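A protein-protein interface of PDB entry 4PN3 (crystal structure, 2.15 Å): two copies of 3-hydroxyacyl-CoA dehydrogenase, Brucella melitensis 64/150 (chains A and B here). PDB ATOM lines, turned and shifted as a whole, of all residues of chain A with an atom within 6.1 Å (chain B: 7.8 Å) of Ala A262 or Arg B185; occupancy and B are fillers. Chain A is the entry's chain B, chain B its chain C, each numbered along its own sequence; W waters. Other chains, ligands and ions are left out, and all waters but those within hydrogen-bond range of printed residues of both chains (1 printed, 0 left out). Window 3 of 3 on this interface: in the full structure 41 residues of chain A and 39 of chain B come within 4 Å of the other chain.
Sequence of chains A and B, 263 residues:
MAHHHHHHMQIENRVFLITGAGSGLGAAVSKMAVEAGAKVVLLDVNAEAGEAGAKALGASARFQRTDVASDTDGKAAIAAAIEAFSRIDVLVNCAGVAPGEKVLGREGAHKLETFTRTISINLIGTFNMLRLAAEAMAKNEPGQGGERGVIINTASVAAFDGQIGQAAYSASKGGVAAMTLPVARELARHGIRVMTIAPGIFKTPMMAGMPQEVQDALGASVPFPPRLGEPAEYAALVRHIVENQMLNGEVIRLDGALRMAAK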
ATOM      1  N   ASP A 161     -11.762 -14.655  16.643  1.00  0.00           N
ATOM      2  CA  ASP A 161     -10.427 -14.376  16.096  1.00  0.00           C
ATOM      3  C   ASP A 161      -9.537 -13.610  17.090  1.00  0.00           C
ATOM      4  O   ASP A 161      -8.798 -12.731  16.688  1.00  0.00           O
ATOM      5  CB  ASP A 161     -10.530 -13.548  14.816  1.00  0.00           C
ATOM      6  CG  ASP A 161     -11.535 -14.103  13.806  1.00  0.00           C
ATOM      7  OD1 ASP A 161     -11.581 -15.346  13.624  1.00  0.00           O
ATOM      8  OD2 ASP A 161     -12.241 -13.289  13.197  1.00  0.00           O
ATOM      9  N   GLY A 162      -9.639 -13.944  18.378  1.00  0.00           N
ATOM     10  CA  GLY A 162      -8.967 -13.210  19.428  1.00  0.00           C
ATOM     11  C   GLY A 162      -7.509 -12.977  19.136  1.00  0.00           C
ATOM     12  O   GLY A 162      -6.787 -13.903  18.746  1.00  0.00           O
ATOM     13  N   GLN A 163      -7.094 -11.722  19.277  1.00  0.00           N
ATOM     14  CA  GLN A 163      -5.711 -11.319  19.049  1.00  0.00           C
ATOM     15  C   GLN A 163      -4.893 -11.469  20.309  1.00  0.00           C
ATOM     16  O   GLN A 163      -5.433 -11.595  21.406  1.00  0.00           O
ATOM     17  CB  GLN A 163      -5.655  -9.859  18.620  1.00  0.00           C
ATOM     18  CG  GLN A 163      -6.500  -9.526  17.396  1.00  0.00           C
ATOM     19  CD  GLN A 163      -6.110  -8.199  16.791  1.00  0.00           C
ATOM     20  OE1 GLN A 163      -6.436  -7.144  17.337  1.00  0.00           O
ATOM     21  NE2 GLN A 163      -5.392  -8.235  15.677  1.00  0.00           N
ATOM     22  N   ILE A 164      -3.579 -11.409  20.142  1.00  0.00           N
ATOM     23  CA  ILE A 164      -2.640 -11.353  21.281  1.00  0.00           C
ATOM     24  C   ILE A 164      -3.026 -10.193  22.183  1.00  0.00           C
ATOM     25  O   ILE A 164      -3.216  -9.068  21.714  1.00  0.00           O
ATOM     26  CB  ILE A 164      -1.201 -11.166  20.789  1.00  0.00           C
ATOM     27  CG1 ILE A 164      -0.717 -12.458  20.118  1.00  0.00           C
ATOM     28  CG2 ILE A 164      -0.279 -10.784  21.926  1.00  0.00           C
ATOM     29  CD1 ILE A 164       0.621 -12.331  19.408  1.00  0.00           C
ATOM     30  N   GLY A 165      -3.230 -10.480  23.472  1.00  0.00           N
ATOM     31  CA  GLY A 165      -3.674  -9.458  24.437  1.00  0.00           C
ATOM     32  C   GLY A 165      -5.179  -9.438  24.725  1.00  0.00           C
ATOM     33  O   GLY A 165      -5.650  -8.651  25.578  1.00  0.00           O
ATOM     34  N   MET A 260      -9.381 -11.119  12.107  1.00  0.00           N
ATOM     35  CA  MET A 260      -8.270 -10.445  12.781  1.00  0.00           C
ATOM     36  C   MET A 260      -7.016 -11.305  12.902  1.00  0.00           C
ATOM     37  O   MET A 260      -7.090 -12.444  13.327  1.00  0.00           O
ATOM     38  CB  MET A 260      -8.691 -10.011  14.186  1.00  0.00           C
ATOM     39  CG  MET A 260      -9.734  -8.921  14.169  1.00  0.00           C
ATOM     40  SD  MET A 260      -9.905  -8.132  15.774  1.00  0.00           S
ATOM     41  CE  MET A 260     -10.339  -9.488  16.869  1.00  0.00           C
ATOM     42  N   ALA A 261      -5.895 -10.764  12.454  1.00  0.00           N
ATOM     43  CA  ALA A 261      -4.583 -11.412  12.604  1.00  0.00           C
ATOM     44  C   ALA A 261      -4.187 -11.367  14.061  1.00  0.00           C
ATOM     45  O   ALA A 261      -4.853 -10.727  14.893  1.00  0.00           O
ATOM     46  CB  ALA A 261      -3.524 -10.699  11.767  1.00  0.00           C
ATOM     47  N   ALA A 262      -3.138 -12.103  14.380  1.00  0.00           N
ATOM     48  CA  ALA A 262      -2.634 -12.241  15.794  1.00  0.00           C
ATOM     49  C   ALA A 262      -2.124 -10.929  16.357  1.00  0.00           C
ATOM     50  O   ALA A 262      -2.303 -10.636  17.554  1.00  0.00           O
ATOM     51  CB  ALA A 262      -1.525 -13.286  15.858  1.00  0.00           C
ATOM     52  N   LYS A 263      -1.471 -10.165  15.478  1.00  0.00           N
ATOM     53  CA  LYS A 263      -0.909  -8.858  15.763  1.00  0.00           C
ATOM     54  C   LYS A 263      -1.799  -7.993  14.857  1.00  0.00           C
ATOM     55  O   LYS A 263      -1.632  -8.071  13.622  1.00  0.00           O
ATOM     56  CB  LYS A 263       0.584  -8.775  15.404  1.00  0.00           C
ATOM     57  OXT LYS A 263      -2.699  -7.284  15.363  1.00  0.00           O
ATOM     58  N   MET B 179     -11.046 -18.247  24.690  1.00  0.00           N
ATOM     59  CA  MET B 179      -9.687 -17.835  25.069  1.00  0.00           C
ATOM     60  C   MET B 179      -8.541 -18.601  24.380  1.00  0.00           C
ATOM     61  O   MET B 179      -7.399 -18.161  24.420  1.00  0.00           O
ATOM     62  CB  MET B 179      -9.420 -18.121  26.545  1.00  0.00           C
ATOM     63  CG  MET B 179     -10.017 -17.159  27.487  1.00  0.00           C
ATOM     64  SD  MET B 179      -9.260 -17.308  29.112  1.00  0.00           S
ATOM     65  CE  MET B 179      -9.492 -19.005  29.620  1.00  0.00           C
ATOM     66  N   THR B 180      -8.826 -19.812  23.935  1.00  0.00           N
ATOM     67  CA  THR B 180      -7.800 -20.720  23.517  1.00  0.00           C
ATOM     68  C   THR B 180      -6.883 -20.069  22.475  1.00  0.00           C
ATOM     69  O   THR B 180      -5.662 -20.111  22.621  1.00  0.00           O
ATOM     70  CB  THR B 180      -8.402 -22.002  22.931  1.00  0.00           C
ATOM     71  OG1 THR B 180      -9.415 -22.498  23.801  1.00  0.00           O
ATOM     72  CG2 THR B 180      -7.306 -23.078  22.773  1.00  0.00           C
ATOM     73  N   LEU B 181      -7.474 -19.484  21.442  1.00  0.00           N
ATOM     74  CA  LEU B 181      -6.703 -18.873  20.341  1.00  0.00           C
ATOM     75  C   LEU B 181      -5.865 -17.634  20.742  1.00  0.00           C
ATOM     76  O   LEU B 181      -4.681 -17.597  20.444  1.00  0.00           O
ATOM     77  CB  LEU B 181      -7.647 -18.515  19.161  1.00  0.00           C
ATOM     78  CG  LEU B 181      -7.021 -17.881  17.922  1.00  0.00           C
ATOM     79  CD1 LEU B 181      -5.929 -18.776  17.313  1.00  0.00           C
ATOM     80  CD2 LEU B 181      -8.101 -17.576  16.926  1.00  0.00           C
ATOM     81  N   PRO B 182      -6.462 -16.629  21.432  1.00  0.00           N
ATOM     82  CA  PRO B 182      -5.638 -15.473  21.770  1.00  0.00           C
ATOM     83  C   PRO B 182      -4.512 -15.812  22.701  1.00  0.00           C
ATOM     84  O   PRO B 182      -3.431 -15.184  22.661  1.00  0.00           O
ATOM     85  CB  PRO B 182      -6.626 -14.488  22.418  1.00  0.00           C
ATOM     86  CG  PRO B 182      -7.839 -15.291  22.740  1.00  0.00           C
ATOM     87  CD  PRO B 182      -7.887 -16.384  21.698  1.00  0.00           C
ATOM     88  N   VAL B 183      -4.756 -16.764  23.585  1.00  0.00           N
ATOM     89  CA  VAL B 183      -3.721 -17.215  24.501  1.00  0.00           C
ATOM     90  C   VAL B 183      -2.645 -17.996  23.714  1.00  0.00           C
ATOM     91  O   VAL B 183      -1.452 -17.739  23.875  1.00  0.00           O
ATOM     92  CB  VAL B 183      -4.310 -18.041  25.662  1.00  0.00           C
ATOM     93  CG1 VAL B 183      -3.198 -18.580  26.563  1.00  0.00           C
ATOM     94  CG2 VAL B 183      -5.218 -17.186  26.520  1.00  0.00           C
ATOM     95  N   ALA B 184      -3.062 -18.923  22.858  1.00  0.00           N
ATOM     96  CA  ALA B 184      -2.111 -19.693  22.072  1.00  0.00           C
ATOM     97  C   ALA B 184      -1.241 -18.791  21.216  1.00  0.00           C
ATOM     98  O   ALA B 184      -0.012 -19.008  21.097  1.00  0.00           O
ATOM     99  CB  ALA B 184      -2.844 -20.705  21.208  1.00  0.00           C
ATOM    100  N   ARG B 185      -1.863 -17.789  20.618  1.00  0.00           N
ATOM    101  CA  ARG B 185      -1.135 -16.842  19.790  1.00  0.00           C
ATOM    102  C   ARG B 185      -0.015 -16.110  20.531  1.00  0.00           C
ATOM    103  O   ARG B 185       1.051 -15.926  19.992  1.00  0.00           O
ATOM    104  CB  ARG B 185      -2.107 -15.814  19.194  1.00  0.00           C
ATOM    105  CG  ARG B 185      -2.911 -16.367  18.027  1.00  0.00           C
ATOM    106  CD  ARG B 185      -4.056 -15.462  17.638  1.00  0.00           C
ATOM    107  NE  ARG B 185      -4.368 -15.625  16.243  1.00  0.00           N
ATOM    108  CZ  ARG B 185      -5.318 -14.964  15.576  1.00  0.00           C
ATOM    109  NH1 ARG B 185      -6.129 -14.082  16.182  1.00  0.00           N
ATOM    110  NH2 ARG B 185      -5.479 -15.224  14.278  1.00  0.00           N
ATOM    111  N   GLU B 186      -0.266 -15.697  21.765  1.00  0.00           N
ATOM    112  CA  GLU B 186       0.757 -14.995  22.528  1.00  0.00           C
ATOM    113  C   GLU B 186       1.826 -15.959  23.035  1.00  0.00           C
ATOM    114  O   GLU B 186       3.022 -15.711  22.875  1.00  0.00           O
ATOM    115  CB  GLU B 186       0.147 -14.285  23.722  1.00  0.00           C
ATOM    116  CG  GLU B 186       1.191 -13.528  24.538  1.00  0.00           C
ATOM    117  CD  GLU B 186       0.679 -13.158  25.904  1.00  0.00           C
ATOM    118  OE1 GLU B 186      -0.560 -12.946  26.028  1.00  0.00           O
ATOM    119  OE2 GLU B 186       1.498 -13.083  26.843  1.00  0.00           O
ATOM    120  N   LEU B 187       1.390 -17.090  23.582  1.00  0.00           N
ATOM    121  CA  LEU B 187       2.315 -17.988  24.252  1.00  0.00           C
ATOM    122  C   LEU B 187       3.158 -18.804  23.264  1.00  0.00           C
ATOM    123  O   LEU B 187       4.126 -19.458  23.673  1.00  0.00           O
ATOM    124  CB  LEU B 187       1.584 -18.901  25.238  1.00  0.00           C
ATOM    125  CG  LEU B 187       0.825 -18.192  26.358  1.00  0.00           C
ATOM    126  CD1 LEU B 187       0.320 -19.232  27.340  1.00  0.00           C
ATOM    127  CD2 LEU B 187       1.675 -17.149  27.086  1.00  0.00           C
ATOM    128  N   ALA B 188       2.798 -18.756  21.989  1.00  0.00           N
ATOM    129  CA  ALA B 188       3.593 -19.346  20.903  1.00  0.00           C
ATOM    130  C   ALA B 188       5.024 -18.826  20.906  1.00  0.00           C
ATOM    131  O   ALA B 188       5.948 -19.574  20.617  1.00  0.00           O
ATOM    132  CB  ALA B 188       2.940 -19.041  19.550  1.00  0.00           C
ATOM    133  N   ARG B 189       5.201 -17.551  21.215  1.00  0.00           N
ATOM    134  CA  ARG B 189       6.518 -16.949  21.250  1.00  0.00           C
ATOM    135  C   ARG B 189       7.444 -17.619  22.291  1.00  0.00           C
ATOM    136  O   ARG B 189       8.667 -17.677  22.107  1.00  0.00           O
ATOM    137  CB  ARG B 189       6.383 -15.452  21.521  1.00  0.00           C
ATOM    138  N   HIS B 190       6.846 -18.163  23.360  1.00  0.00           N
ATOM    139  CA  HIS B 190       7.593 -18.922  24.376  1.00  0.00           C
ATOM    140  C   HIS B 190       7.579 -20.434  24.185  1.00  0.00           C
ATOM    141  O   HIS B 190       8.078 -21.163  25.013  1.00  0.00           O
ATOM    142  CB  HIS B 190       6.990 -18.663  25.756  1.00  0.00           C
ATOM    143  CG  HIS B 190       6.784 -17.221  26.092  1.00  0.00           C
ATOM    144  ND1 HIS B 190       7.767 -16.440  26.655  1.00  0.00           N
ATOM    145  CD2 HIS B 190       5.711 -16.420  25.940  1.00  0.00           C
ATOM    146  CE1 HIS B 190       7.303 -15.218  26.842  1.00  0.00           C
ATOM    147  NE2 HIS B 190       6.058 -15.181  26.421  1.00  0.00           N
ATOM    148  N   ILE B 192       4.885 -22.353  24.289  1.00  0.00           N
ATOM    149  CA  ILE B 192       3.850 -22.943  25.129  1.00  0.00           C
ATOM    150  C   ILE B 192       2.560 -23.111  24.305  1.00  0.00           C
ATOM    151  O   ILE B 192       2.013 -22.122  23.793  1.00  0.00           O
ATOM    152  CB  ILE B 192       3.540 -22.072  26.362  1.00  0.00           C
ATOM    153  CG1 ILE B 192       4.767 -21.946  27.255  1.00  0.00           C
ATOM    154  CG2 ILE B 192       2.375 -22.668  27.144  1.00  0.00           C
ATOM    155  CD1 ILE B 192       4.663 -20.830  28.285  1.00  0.00           C
ATOM    156  N   VAL B 194      -1.434 -24.270  23.708  1.00  0.00           N
ATOM    157  CA  VAL B 194      -2.668 -24.105  24.449  1.00  0.00           C
ATOM    158  C   VAL B 194      -3.809 -24.770  23.691  1.00  0.00           C
ATOM    159  O   VAL B 194      -4.109 -24.397  22.573  1.00  0.00           O
ATOM    160  CB  VAL B 194      -2.988 -22.620  24.667  1.00  0.00           C
ATOM    161  CG1 VAL B 194      -4.224 -22.464  25.561  1.00  0.00           C
ATOM    162  CG2 VAL B 194      -1.815 -21.914  25.313  1.00  0.00           C
ATOM    163  N   ASN B 248      -2.567 -27.410  18.498  1.00  0.00           N
ATOM    164  CA  ASN B 248      -2.489 -26.108  19.148  1.00  0.00           C
ATOM    165  C   ASN B 248      -3.626 -25.182  18.752  1.00  0.00           C
ATOM    166  O   ASN B 248      -4.029 -25.138  17.583  1.00  0.00           O
ATOM    167  CB  ASN B 248      -1.145 -25.428  18.863  1.00  0.00           C
ATOM    168  CG  ASN B 248      -0.828 -24.289  19.838  1.00  0.00           C
ATOM    169  OD1 ASN B 248      -1.377 -24.220  20.946  1.00  0.00           O
ATOM    170  ND2 ASN B 248       0.147 -23.492  19.492  1.00  0.00           N
ATOM    171  N   GLY B 249      -4.133 -24.458  19.754  1.00  0.00           N
ATOM    172  CA  GLY B 249      -5.120 -23.389  19.543  1.00  0.00           C
ATOM    173  C   GLY B 249      -6.493 -23.849  19.121  1.00  0.00           C
ATOM    174  O   GLY B 249      -7.259 -23.084  18.541  1.00  0.00           O
HETATM  175  O   HOH W   1      -2.795 -13.175  24.948  1.00  0.00           O
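O of Asp A161 sits at hydrogen-bond distance from NH1 of Arg B185, 3.0 Å away.
O of Gly A162 is in hydrogen-bond range of NH1 of Arg B185 (2.7 Å).
NH2 of Arg B185 is in hydrogen-bond range of O of Met A260 (3.4 Å).
The side-chain amide nitrogen (NE2) of Gln A163 sits at hydrogen-bond distance from the backbone carbonyl oxygen (O) of Ala A261.
The chain-end carboxylate (OXT) of Lys A263 sits at hydrogen-bond distance from the side-chain amide nitrogen (NE2) of Gln A163.
The backbone NH of Ile A164 sits at hydrogen-bond distance from the backbone carbonyl oxygen of Ala A262 (3.0 Å).
Among the printed residues, merely in contact across the chains: Gly A162 with Pro B182 (3.6 Å), Gln A163 with Pro B182 (3.3 Å), Ile A164 with Arg B185 (3.7 Å), Ile A164 with Glu B186 (3.7 Å), Ala A261 with Arg B185 (3.8 Å) and Ala A262 with Arg B185 (3.7 Å).
Of the printed residues of chain B, Asp A161 touches Arg B185 (3.0 Å).
Of the printed residues of chain B, Gly A162 touches Pro B182 (3.6 Å) and Arg B185 (2.7 Å).
Of the printed residues of chain B, Gln A163 touches Pro B182.
Printed residues of chain B within 4 Å of Ile A164: Arg B185 (3.7 Å) and Glu B186 (3.7 Å).
Ala A261 touches one residue of chain B.
Of chain B, only Arg B185 comes within 4 Å of Ala A262.
Ala B184 touches none of the printed residues of chain A.
Asn B248 touches none of the printed residues of chain A.
The nearest residue of chain B that does not touch Ala A262 is Glu B186 (6.5 Å).
Of the 9 printed residues of chain A, 7 touch a printed residue of chain B.
Hydrophobic or aromatic side chains of chain A within 4 Å of the printed part of chain B: Ile A164 and Ala A262.
Among the printed residues, 9 pairs touch across the chains.
No position is printed for both chains.
Of the 9 pairs that touch across the chains among the printed residues, none has its exchanged pair printed and touching as well.
Water W1 lies within hydrogen-bond range of OE1 of Glu B186 (2.5 Å), N of Gly A165 (3.1 Å) and O of Pro B182 (3.1 Å).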
